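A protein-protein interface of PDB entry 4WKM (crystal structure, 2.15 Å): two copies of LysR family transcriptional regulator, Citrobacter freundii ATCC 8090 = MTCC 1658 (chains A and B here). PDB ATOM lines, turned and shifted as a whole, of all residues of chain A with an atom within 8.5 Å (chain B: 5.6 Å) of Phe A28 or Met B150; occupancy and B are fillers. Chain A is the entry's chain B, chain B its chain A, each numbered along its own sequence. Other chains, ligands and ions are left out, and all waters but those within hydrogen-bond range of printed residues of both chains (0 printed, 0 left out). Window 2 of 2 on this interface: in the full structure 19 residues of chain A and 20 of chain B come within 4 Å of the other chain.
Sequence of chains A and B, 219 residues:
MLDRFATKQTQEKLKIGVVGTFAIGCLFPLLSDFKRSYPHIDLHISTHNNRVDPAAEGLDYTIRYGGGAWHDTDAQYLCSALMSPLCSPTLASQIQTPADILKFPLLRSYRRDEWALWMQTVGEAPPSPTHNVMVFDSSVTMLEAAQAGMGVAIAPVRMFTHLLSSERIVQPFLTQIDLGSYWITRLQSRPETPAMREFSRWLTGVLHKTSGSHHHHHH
The backbone carbonyl oxygen of Ala B145 is in hydrogen-bond range of the backbone NH of Met B150 (3.1 Å).
The backbone carbonyl oxygen of Ala A23 is in hydrogen-bond range of the backbone NH of Phe A28, 2.9 Å away.
Among the printed residues, merely in contact across the chains: Thr A47 with Phe B136 (3.4 Å), Ile A24 with Ala B145 (3.5 Å), Phe A28 with Met B150 (3.6 Å), Ile A45 with Met B134 (3.6 Å), Phe A28 with Ala B145 (3.8 Å), Phe A28 with Met B134 (3.8 Å) and Phe A28 with Phe B136 (3.9 Å).
Leu A27 touches none of the printed residues of chain B.
Of the printed residues of chain B, Phe A28 touches Met B134, Phe B136, Ala B145 and Met B150.
Of the printed residues of chain B, Ile A45 touches Met B134 (3.6 Å).
Of the printed residues of chain B, Thr A47 touches Phe B136.
Leu B91 touches none of the printed residues of chain A.
Printed residues of chain A within 4 Å of Phe B136: Phe A28 (3.9 Å) and Thr A47 (3.4 Å).
Gly B149 touches none of the printed residues of chain A.
No residue of chain A comes within 4 Å of Gly B151.
The nearest printed residue of chain B that does not touch Phe A28 is Ala B148 (6.2 Å).
The nearest printed residue of chain A that does not touch Phe B136 is Ile A24 (5.1 Å).
Hydrophobic or aromatic side chains of chain B that line the printed part of chain A: Met B134, Phe B136, Ala B145 and Met B150.
Of the 24 printed residues of chain A, 4 touch a printed residue of chain B.
Printed residues of chain A that touch a printed residue of chain B: Ile A24, Phe A28, Ile A45 and Thr A47.
Among the printed residues, no Asp or Glu carboxylate lies within 4 Å of a Lys or Arg side-chain nitrogen of the other chain.
No position is printed for both chains.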
ATOM      1  N   ILE A  16      25.960  -5.334   9.364  1.00  0.00           N
ATOM      2  CA  ILE A  16      26.525  -5.890  10.597  1.00  0.00           C
ATOM      3  C   ILE A  16      27.248  -7.210  10.374  1.00  0.00           C
ATOM      4  O   ILE A  16      26.643  -8.154   9.873  1.00  0.00           O
ATOM      5  CB  ILE A  16      25.390  -6.107  11.643  1.00  0.00           C
ATOM      6  CG1 ILE A  16      24.784  -4.739  11.984  1.00  0.00           C
ATOM      7  CG2 ILE A  16      25.891  -6.831  12.929  1.00  0.00           C
ATOM      8  CD1 ILE A  16      23.708  -4.772  13.004  1.00  0.00           C
ATOM      9  N   VAL A  18      28.760 -10.466  12.213  1.00  0.00           N
ATOM     10  CA  VAL A  18      28.454 -11.214  13.446  1.00  0.00           C
ATOM     11  C   VAL A  18      29.229 -12.525  13.588  1.00  0.00           C
ATOM     12  O   VAL A  18      29.141 -13.437  12.701  1.00  0.00           O
ATOM     13  CB  VAL A  18      26.969 -11.579  13.506  1.00  0.00           C
ATOM     14  CG1 VAL A  18      26.603 -12.091  14.841  1.00  0.00           C
ATOM     15  CG2 VAL A  18      26.137 -10.395  13.185  1.00  0.00           C
ATOM     16  N   VAL A  19      29.956 -12.656  14.696  1.00  0.00           N
ATOM     17  CA  VAL A  19      30.681 -13.892  14.925  1.00  0.00           C
ATOM     18  C   VAL A  19      29.666 -15.030  14.840  1.00  0.00           C
ATOM     19  O   VAL A  19      28.557 -14.922  15.347  1.00  0.00           O
ATOM     20  CB  VAL A  19      31.469 -13.917  16.256  1.00  0.00           C
ATOM     21  CG1 VAL A  19      30.554 -13.688  17.517  1.00  0.00           C
ATOM     22  CG2 VAL A  19      32.250 -15.240  16.352  1.00  0.00           C
ATOM     23  N   GLY A  20      30.024 -16.099  14.121  1.00  0.00           N
ATOM     24  CA  GLY A  20      29.050 -17.105  13.693  1.00  0.00           C
ATOM     25  C   GLY A  20      28.332 -17.838  14.802  1.00  0.00           C
ATOM     26  O   GLY A  20      27.155 -18.210  14.676  1.00  0.00           O
ATOM     27  N   THR A  21      29.058 -18.085  15.885  1.00  0.00           N
ATOM     28  CA  THR A  21      28.466 -18.617  17.098  1.00  0.00           C
ATOM     29  C   THR A  21      27.309 -17.789  17.608  1.00  0.00           C
ATOM     30  O   THR A  21      26.258 -18.329  17.980  1.00  0.00           O
ATOM     31  CB  THR A  21      29.509 -18.688  18.205  1.00  0.00           C
ATOM     32  OG1 THR A  21      30.640 -19.368  17.675  1.00  0.00           O
ATOM     33  CG2 THR A  21      28.958 -19.426  19.411  1.00  0.00           C
ATOM     34  N   PHE A  22      27.525 -16.477  17.660  1.00  0.00           N
ATOM     35  CA  PHE A  22      26.508 -15.557  18.160  1.00  0.00           C
ATOM     36  C   PHE A  22      25.359 -15.515  17.163  1.00  0.00           C
ATOM     37  O   PHE A  22      24.207 -15.579  17.541  1.00  0.00           O
ATOM     38  CB  PHE A  22      27.113 -14.165  18.368  1.00  0.00           C
ATOM     39  CG  PHE A  22      26.188 -13.181  19.069  1.00  0.00           C
ATOM     40  CD1 PHE A  22      26.075 -13.167  20.455  1.00  0.00           C
ATOM     41  CD2 PHE A  22      25.462 -12.249  18.334  1.00  0.00           C
ATOM     42  CE1 PHE A  22      25.237 -12.232  21.103  1.00  0.00           C
ATOM     43  CE2 PHE A  22      24.640 -11.319  18.953  1.00  0.00           C
ATOM     44  CZ  PHE A  22      24.515 -11.306  20.347  1.00  0.00           C
ATOM     45  N   ALA A  23      25.681 -15.438  15.873  1.00  0.00           N
ATOM     46  CA  ALA A  23      24.628 -15.408  14.871  1.00  0.00           C
ATOM     47  C   ALA A  23      23.715 -16.609  15.057  1.00  0.00           C
ATOM     48  O   ALA A  23      22.504 -16.471  15.141  1.00  0.00           O
ATOM     49  CB  ALA A  23      25.227 -15.364  13.465  1.00  0.00           C
ATOM     50  N   ILE A  24      24.290 -17.794  15.183  1.00  0.00           N
ATOM     51  CA  ILE A  24      23.480 -18.999  15.289  1.00  0.00           C
ATOM     52  C   ILE A  24      22.799 -19.174  16.660  1.00  0.00           C
ATOM     53  O   ILE A  24      21.650 -19.610  16.745  1.00  0.00           O
ATOM     54  CB  ILE A  24      24.334 -20.261  15.033  1.00  0.00           C
ATOM     55  CG1 ILE A  24      24.940 -20.251  13.611  1.00  0.00           C
ATOM     56  CG2 ILE A  24      23.526 -21.498  15.324  1.00  0.00           C
ATOM     57  CD1 ILE A  24      23.934 -20.411  12.460  1.00  0.00           C
ATOM     58  N   GLY A  25      23.521 -18.910  17.744  1.00  0.00           N
ATOM     59  CA  GLY A  25      22.995 -19.227  19.069  1.00  0.00           C
ATOM     60  C   GLY A  25      22.077 -18.181  19.686  1.00  0.00           C
ATOM     61  O   GLY A  25      21.221 -18.490  20.512  1.00  0.00           O
ATOM     62  N   CYS A  26      22.249 -16.946  19.268  1.00  0.00           N
ATOM     63  CA  CYS A  26      21.559 -15.832  19.884  1.00  0.00           C
ATOM     64  C   CYS A  26      20.781 -14.998  18.859  1.00  0.00           C
ATOM     65  O   CYS A  26      19.555 -14.944  18.894  1.00  0.00           O
ATOM     66  CB  CYS A  26      22.576 -14.967  20.626  1.00  0.00           C
ATOM     67  SG  CYS A  26      21.844 -13.594  21.527  1.00  0.00           S
ATOM     68  N   LEU A  27      21.487 -14.369  17.934  1.00  0.00           N
ATOM     69  CA  LEU A  27      20.855 -13.387  17.053  1.00  0.00           C
ATOM     70  C   LEU A  27      19.797 -13.921  16.099  1.00  0.00           C
ATOM     71  O   LEU A  27      18.746 -13.321  15.971  1.00  0.00           O
ATOM     72  CB  LEU A  27      21.909 -12.675  16.241  1.00  0.00           C
ATOM     73  CG  LEU A  27      21.374 -11.568  15.335  1.00  0.00           C
ATOM     74  CD1 LEU A  27      20.712 -10.476  16.109  1.00  0.00           C
ATOM     75  CD2 LEU A  27      22.510 -11.001  14.574  1.00  0.00           C
ATOM     76  N   PHE A  28      20.046 -15.035  15.430  1.00  0.00           N
ATOM     77  CA  PHE A  28      19.178 -15.411  14.328  1.00  0.00           C
ATOM     78  C   PHE A  28      17.787 -15.674  14.832  1.00  0.00           C
ATOM     79  O   PHE A  28      16.830 -15.229  14.208  1.00  0.00           O
ATOM     80  CB  PHE A  28      19.718 -16.639  13.554  1.00  0.00           C
ATOM     81  CG  PHE A  28      20.775 -16.299  12.527  1.00  0.00           C
ATOM     82  CD1 PHE A  28      21.050 -14.995  12.197  1.00  0.00           C
ATOM     83  CD2 PHE A  28      21.499 -17.302  11.907  1.00  0.00           C
ATOM     84  CE1 PHE A  28      22.012 -14.674  11.263  1.00  0.00           C
ATOM     85  CE2 PHE A  28      22.462 -16.997  10.964  1.00  0.00           C
ATOM     86  CZ  PHE A  28      22.728 -15.685  10.640  1.00  0.00           C
ATOM     87  N   PRO A  29      17.661 -16.397  15.958  1.00  0.00           N
ATOM     88  CA  PRO A  29      16.322 -16.566  16.532  1.00  0.00           C
ATOM     89  C   PRO A  29      15.594 -15.247  16.808  1.00  0.00           C
ATOM     90  O   PRO A  29      14.369 -15.241  16.851  1.00  0.00           O
ATOM     91  CB  PRO A  29      16.602 -17.324  17.832  1.00  0.00           C
ATOM     92  CG  PRO A  29      17.766 -18.164  17.493  1.00  0.00           C
ATOM     93  CD  PRO A  29      18.630 -17.320  16.575  1.00  0.00           C
ATOM     94  N   LEU A  30      16.327 -14.149  16.949  1.00  0.00           N
ATOM     95  CA  LEU A  30      15.720 -12.888  17.359  1.00  0.00           C
ATOM     96  C   LEU A  30      15.423 -11.945  16.198  1.00  0.00           C
ATOM     97  O   LEU A  30      14.812 -10.903  16.391  1.00  0.00           O
ATOM     98  CB  LEU A  30      16.629 -12.181  18.362  1.00  0.00           C
ATOM     99  CG  LEU A  30      16.918 -12.981  19.637  1.00  0.00           C
ATOM    100  CD1 LEU A  30      17.824 -12.174  20.518  1.00  0.00           C
ATOM    101  CD2 LEU A  30      15.670 -13.366  20.388  1.00  0.00           C
ATOM    102  N   LEU A  31      15.828 -12.306  14.989  1.00  0.00           N
ATOM    103  CA  LEU A  31      15.752 -11.354  13.882  1.00  0.00           C
ATOM    104  C   LEU A  31      14.320 -11.103  13.380  1.00  0.00           C
ATOM    105  O   LEU A  31      14.065 -10.075  12.755  1.00  0.00           O
ATOM    106  CB  LEU A  31      16.615 -11.835  12.721  1.00  0.00           C
ATOM    107  CG  LEU A  31      18.124 -11.715  12.890  1.00  0.00           C
ATOM    108  CD1 LEU A  31      18.808 -12.386  11.704  1.00  0.00           C
ATOM    109  CD2 LEU A  31      18.565 -10.279  13.012  1.00  0.00           C
ATOM    110  N   SER A  32      13.399 -12.032  13.641  1.00  0.00           N
ATOM    111  CA  SER A  32      11.999 -11.847  13.267  1.00  0.00           C
ATOM    112  C   SER A  32      11.331 -10.826  14.192  1.00  0.00           C
ATOM    113  O   SER A  32      10.355 -10.183  13.823  1.00  0.00           O
ATOM    114  CB  SER A  32      11.254 -13.164  13.322  1.00  0.00           C
ATOM    115  OG  SER A  32      11.565 -13.825  14.531  1.00  0.00           O
ATOM    116  N   ASP A  33      11.866 -10.693  15.402  1.00  0.00           N
ATOM    117  CA  ASP A  33      11.431  -9.653  16.326  1.00  0.00           C
ATOM    118  C   ASP A  33      11.907  -8.305  15.799  1.00  0.00           C
ATOM    119  O   ASP A  33      11.163  -7.337  15.804  1.00  0.00           O
ATOM    120  CB  ASP A  33      11.970  -9.922  17.746  1.00  0.00           C
ATOM    121  CG  ASP A  33      11.235  -9.120  18.830  1.00  0.00           C
ATOM    122  OD1 ASP A  33      10.100  -9.512  19.190  1.00  0.00           O
ATOM    123  OD2 ASP A  33      11.797  -8.117  19.338  1.00  0.00           O
ATOM    124  N   PHE A  34      13.144  -8.232  15.324  1.00  0.00           N
ATOM    125  CA  PHE A  34      13.651  -6.973  14.785  1.00  0.00           C
ATOM    126  C   PHE A  34      13.036  -6.691  13.429  1.00  0.00           C
ATOM    127  O   PHE A  34      13.212  -5.604  12.879  1.00  0.00           O
ATOM    128  CB  PHE A  34      15.172  -7.002  14.660  1.00  0.00           C
ATOM    129  CG  PHE A  34      15.768  -5.735  14.097  1.00  0.00           C
ATOM    130  CD1 PHE A  34      15.901  -4.604  14.886  1.00  0.00           C
ATOM    131  CD2 PHE A  34      16.209  -5.680  12.782  1.00  0.00           C
ATOM    132  CE1 PHE A  34      16.453  -3.444  14.380  1.00  0.00           C
ATOM    133  CE2 PHE A  34      16.772  -4.514  12.263  1.00  0.00           C
ATOM    134  CZ  PHE A  34      16.894  -3.397  13.062  1.00  0.00           C
ATOM    135  N   LEU A  43      18.546  -4.858   6.963  1.00  0.00           N
ATOM    136  CA  LEU A  43      19.679  -5.466   7.667  1.00  0.00           C
ATOM    137  C   LEU A  43      20.562  -6.385   6.776  1.00  0.00           C
ATOM    138  O   LEU A  43      20.115  -7.453   6.352  1.00  0.00           O
ATOM    139  CB  LEU A  43      19.118  -6.257   8.860  1.00  0.00           C
ATOM    140  CG  LEU A  43      20.025  -6.675  10.016  1.00  0.00           C
ATOM    141  CD1 LEU A  43      20.991  -5.574  10.436  1.00  0.00           C
ATOM    142  CD2 LEU A  43      19.155  -7.061  11.179  1.00  0.00           C
ATOM    143  N   ILE A  45      23.342  -8.871   7.031  1.00  0.00           N
ATOM    144  CA  ILE A  45      24.111  -9.703   7.987  1.00  0.00           C
ATOM    145  C   ILE A  45      25.176 -10.584   7.325  1.00  0.00           C
ATOM    146  O   ILE A  45      24.870 -11.402   6.440  1.00  0.00           O
ATOM    147  CB  ILE A  45      23.180 -10.624   8.802  1.00  0.00           C
ATOM    148  CG1 ILE A  45      22.103  -9.799   9.512  1.00  0.00           C
ATOM    149  CG2 ILE A  45      23.975 -11.446   9.863  1.00  0.00           C
ATOM    150  CD1 ILE A  45      21.091 -10.657  10.248  1.00  0.00           C
ATOM    151  N   SER A  46      26.423 -10.412   7.758  1.00  0.00           N
ATOM    152  CA  SER A  46      27.492 -11.338   7.411  1.00  0.00           C
ATOM    153  C   SER A  46      28.106 -11.953   8.653  1.00  0.00           C
ATOM    154  O   SER A  46      28.071 -11.326   9.727  1.00  0.00           O
ATOM    155  CB  SER A  46      28.565 -10.656   6.576  1.00  0.00           C
ATOM    156  OG  SER A  46      29.216  -9.611   7.245  1.00  0.00           O
ATOM    157  N   THR A  47      28.614 -13.193   8.524  1.00  0.00           N
ATOM    158  CA  THR A  47      29.283 -13.872   9.642  1.00  0.00           C
ATOM    159  C   THR A  47      30.786 -13.889   9.467  1.00  0.00           C
ATOM    160  O   THR A  47      31.303 -13.810   8.340  1.00  0.00           O
ATOM    161  CB  THR A  47      28.814 -15.329   9.862  1.00  0.00           C
ATOM    162  OG1 THR A  47      29.398 -16.213   8.879  1.00  0.00           O
ATOM    163  CG2 THR A  47      27.317 -15.409   9.861  1.00  0.00           C
ATOM    164  N   TRP A 202      17.648  -2.167  20.392  1.00  0.00           N
ATOM    165  CA  TRP A 202      16.744  -3.327  20.345  1.00  0.00           C
ATOM    166  C   TRP A 202      17.424  -4.578  20.859  1.00  0.00           C
ATOM    167  O   TRP A 202      16.792  -5.395  21.534  1.00  0.00           O
ATOM    168  CB  TRP A 202      16.226  -3.604  18.926  1.00  0.00           C
ATOM    169  CG  TRP A 202      15.657  -4.978  18.803  1.00  0.00           C
ATOM    170  CD1 TRP A 202      14.420  -5.393  19.209  1.00  0.00           C
ATOM    171  CD2 TRP A 202      16.313  -6.140  18.270  1.00  0.00           C
ATOM    172  NE1 TRP A 202      14.260  -6.747  18.961  1.00  0.00           N
ATOM    173  CE2 TRP A 202      15.408  -7.221  18.378  1.00  0.00           C
ATOM    174  CE3 TRP A 202      17.572  -6.372  17.710  1.00  0.00           C
ATOM    175  CZ2 TRP A 202      15.725  -8.505  17.938  1.00  0.00           C
ATOM    176  CZ3 TRP A 202      17.882  -7.654  17.282  1.00  0.00           C
ATOM    177  CH2 TRP A 202      16.964  -8.698  17.397  1.00  0.00           C
ATOM    178  N   LEU A 203      18.712  -4.726  20.539  1.00  0.00           N
ATOM    179  CA  LEU A 203      19.433  -5.972  20.828  1.00  0.00           C
ATOM    180  C   LEU A 203      19.866  -6.044  22.294  1.00  0.00           C
ATOM    181  O   LEU A 203      19.628  -7.060  22.971  1.00  0.00           O
ATOM    182  CB  LEU A 203      20.655  -6.115  19.916  1.00  0.00           C
ATOM    183  CG  LEU A 203      21.462  -7.402  20.101  1.00  0.00           C
ATOM    184  CD1 LEU A 203      20.595  -8.637  19.941  1.00  0.00           C
ATOM    185  CD2 LEU A 203      22.645  -7.452  19.141  1.00  0.00           C
ATOM    186  N   LEU B  91      11.208 -25.946   4.658  1.00  0.00           N
ATOM    187  CA  LEU B  91      11.231 -25.114   3.469  1.00  0.00           C
ATOM    188  C   LEU B  91      11.090 -25.977   2.219  1.00  0.00           C
ATOM    189  O   LEU B  91      10.434 -25.579   1.251  1.00  0.00           O
ATOM    190  CB  LEU B  91      12.518 -24.305   3.408  1.00  0.00           C
ATOM    191  CG  LEU B  91      12.505 -22.963   4.115  1.00  0.00           C
ATOM    192  CD1 LEU B  91      12.305 -23.112   5.643  1.00  0.00           C
ATOM    193  CD2 LEU B  91      13.791 -22.238   3.795  1.00  0.00           C
ATOM    194  N   PRO B 105      14.889 -16.360   1.876  1.00  0.00           N
ATOM    195  CA  PRO B 105      16.169 -15.661   1.764  1.00  0.00           C
ATOM    196  C   PRO B 105      17.254 -16.586   1.234  1.00  0.00           C
ATOM    197  O   PRO B 105      17.161 -17.784   1.411  1.00  0.00           O
ATOM    198  CB  PRO B 105      16.458 -15.240   3.207  1.00  0.00           C
ATOM    199  CG  PRO B 105      15.138 -15.288   3.882  1.00  0.00           C
ATOM    200  CD  PRO B 105      14.413 -16.393   3.269  1.00  0.00           C
ATOM    201  N   LEU B 107      21.101 -17.984   1.320  1.00  0.00           N
ATOM    202  CA  LEU B 107      22.360 -17.986   2.052  1.00  0.00           C
ATOM    203  C   LEU B 107      23.485 -18.242   1.065  1.00  0.00           C
ATOM    204  O   LEU B 107      23.404 -19.146   0.253  1.00  0.00           O
ATOM    205  CB  LEU B 107      22.335 -19.032   3.179  1.00  0.00           C
ATOM    206  CG  LEU B 107      20.991 -19.093   3.919  1.00  0.00           C
ATOM    207  CD1 LEU B 107      21.002 -20.158   4.974  1.00  0.00           C
ATOM    208  CD2 LEU B 107      20.635 -17.757   4.534  1.00  0.00           C
ATOM    209  N   ASN B 132      16.532 -10.895  -0.322  1.00  0.00           N
ATOM    210  CA  ASN B 132      17.098 -11.084   1.028  1.00  0.00           C
ATOM    211  C   ASN B 132      18.213 -12.133   1.029  1.00  0.00           C
ATOM    212  O   ASN B 132      17.959 -13.312   0.763  1.00  0.00           O
ATOM    213  CB  ASN B 132      15.988 -11.492   1.988  1.00  0.00           C
ATOM    214  CG  ASN B 132      16.400 -11.416   3.427  1.00  0.00           C
ATOM    215  OD1 ASN B 132      16.020 -12.274   4.235  1.00  0.00           O
ATOM    216  ND2 ASN B 132      17.175 -10.387   3.775  1.00  0.00           N
ATOM    217  N   MET B 134      21.912 -13.514   3.171  1.00  0.00           N
ATOM    218  CA  MET B 134      22.919 -13.480   4.236  1.00  0.00           C
ATOM    219  C   MET B 134      24.234 -14.114   3.777  1.00  0.00           C
ATOM    220  O   MET B 134      24.224 -15.146   3.121  1.00  0.00           O
ATOM    221  CB  MET B 134      22.401 -14.202   5.467  1.00  0.00           C
ATOM    222  CG  MET B 134      21.126 -13.614   6.007  1.00  0.00           C
ATOM    223  SD  MET B 134      20.860 -14.009   7.721  1.00  0.00           S
ATOM    224  CE  MET B 134      19.989 -15.552   7.523  1.00  0.00           C
ATOM    225  N   PHE B 136      27.971 -15.817   4.606  1.00  0.00           N
ATOM    226  CA  PHE B 136      28.618 -16.698   5.570  1.00  0.00           C
ATOM    227  C   PHE B 136      30.083 -16.924   5.244  1.00  0.00           C
ATOM    228  O   PHE B 136      30.474 -17.016   4.066  1.00  0.00           O
ATOM    229  CB  PHE B 136      27.880 -18.005   5.623  1.00  0.00           C
ATOM    230  CG  PHE B 136      26.513 -17.900   6.234  1.00  0.00           C
ATOM    231  CD1 PHE B 136      26.336 -17.999   7.604  1.00  0.00           C
ATOM    232  CD2 PHE B 136      25.414 -17.661   5.449  1.00  0.00           C
ATOM    233  CE1 PHE B 136      25.089 -17.906   8.159  1.00  0.00           C
ATOM    234  CE2 PHE B 136      24.148 -17.566   6.003  1.00  0.00           C
ATOM    235  CZ  PHE B 136      23.989 -17.683   7.363  1.00  0.00           C
ATOM    236  N   ALA B 145      22.416 -22.317   9.950  1.00  0.00           N
ATOM    237  CA  ALA B 145      21.394 -21.339   9.667  1.00  0.00           C
ATOM    238  C   ALA B 145      20.277 -21.926   8.814  1.00  0.00           C
ATOM    239  O   ALA B 145      19.102 -21.603   9.010  1.00  0.00           O
ATOM    240  CB  ALA B 145      22.011 -20.163   8.998  1.00  0.00           C
ATOM    241  N   ALA B 146      20.619 -22.801   7.870  1.00  0.00           N
ATOM    242  CA  ALA B 146      19.586 -23.390   6.997  1.00  0.00           C
ATOM    243  C   ALA B 146      18.744 -24.400   7.769  1.00  0.00           C
ATOM    244  O   ALA B 146      17.542 -24.536   7.523  1.00  0.00           O
ATOM    245  CB  ALA B 146      20.219 -24.055   5.750  1.00  0.00           C
ATOM    246  N   ALA B 148      17.791 -24.127  10.661  1.00  0.00           N
ATOM    247  CA  ALA B 148      16.924 -23.324  11.515  1.00  0.00           C
ATOM    248  C   ALA B 148      15.926 -22.508  10.678  1.00  0.00           C
ATOM    249  O   ALA B 148      15.139 -21.744  11.208  1.00  0.00           O
ATOM    250  CB  ALA B 148      17.778 -22.399  12.374  1.00  0.00           C
ATOM    251  N   GLY B 149      16.013 -22.636   9.358  1.00  0.00           N
ATOM    252  CA  GLY B 149      15.018 -22.076   8.461  1.00  0.00           C
ATOM    253  C   GLY B 149      15.238 -20.626   8.153  1.00  0.00           C
ATOM    254  O   GLY B 149      14.314 -19.929   7.761  1.00  0.00           O
ATOM    255  N   MET B 150      16.471 -20.171   8.295  1.00  0.00           N
ATOM    256  CA  MET B 150      16.806 -18.805   7.967  1.00  0.00           C
ATOM    257  C   MET B 150      16.773 -18.501   6.463  1.00  0.00           C
ATOM    258  O   MET B 150      16.761 -17.320   6.062  1.00  0.00           O
ATOM    259  CB  MET B 150      18.189 -18.479   8.531  1.00  0.00           C
ATOM    260  CG  MET B 150      18.269 -18.784  10.043  1.00  0.00           C
ATOM    261  SD  MET B 150      16.962 -17.875  10.934  1.00  0.00           S
ATOM    262  CE  MET B 150      17.543 -16.181  10.735  1.00  0.00           C
ATOM    263  N   GLY B 151      16.724 -19.549   5.641  1.00  0.00           N
ATOM    264  CA  GLY B 151      16.964 -19.385   4.219  1.00  0.00           C
ATOM    265  C   GLY B 151      17.456 -20.646   3.567  1.00  0.00           C
ATOM    266  O   GLY B 151      17.538 -21.712   4.211  1.00  0.00           O
ATOM    267  N   VAL B 152      17.782 -20.536   2.286  1.00  0.00           N
ATOM    268  CA  VAL B 152      18.215 -21.715   1.523  1.00  0.00           C
ATOM    269  C   VAL B 152      19.714 -21.627   1.275  1.00  0.00           C
ATOM    270  O   VAL B 152      20.212 -20.617   0.779  1.00  0.00           O
ATOM    271  CB  VAL B 152      17.431 -21.862   0.194  1.00  0.00           C
ATOM    272  CG1 VAL B 152      18.065 -22.924  -0.694  1.00  0.00           C
ATOM    273  CG2 VAL B 152      15.955 -22.197   0.500  1.00  0.00           C
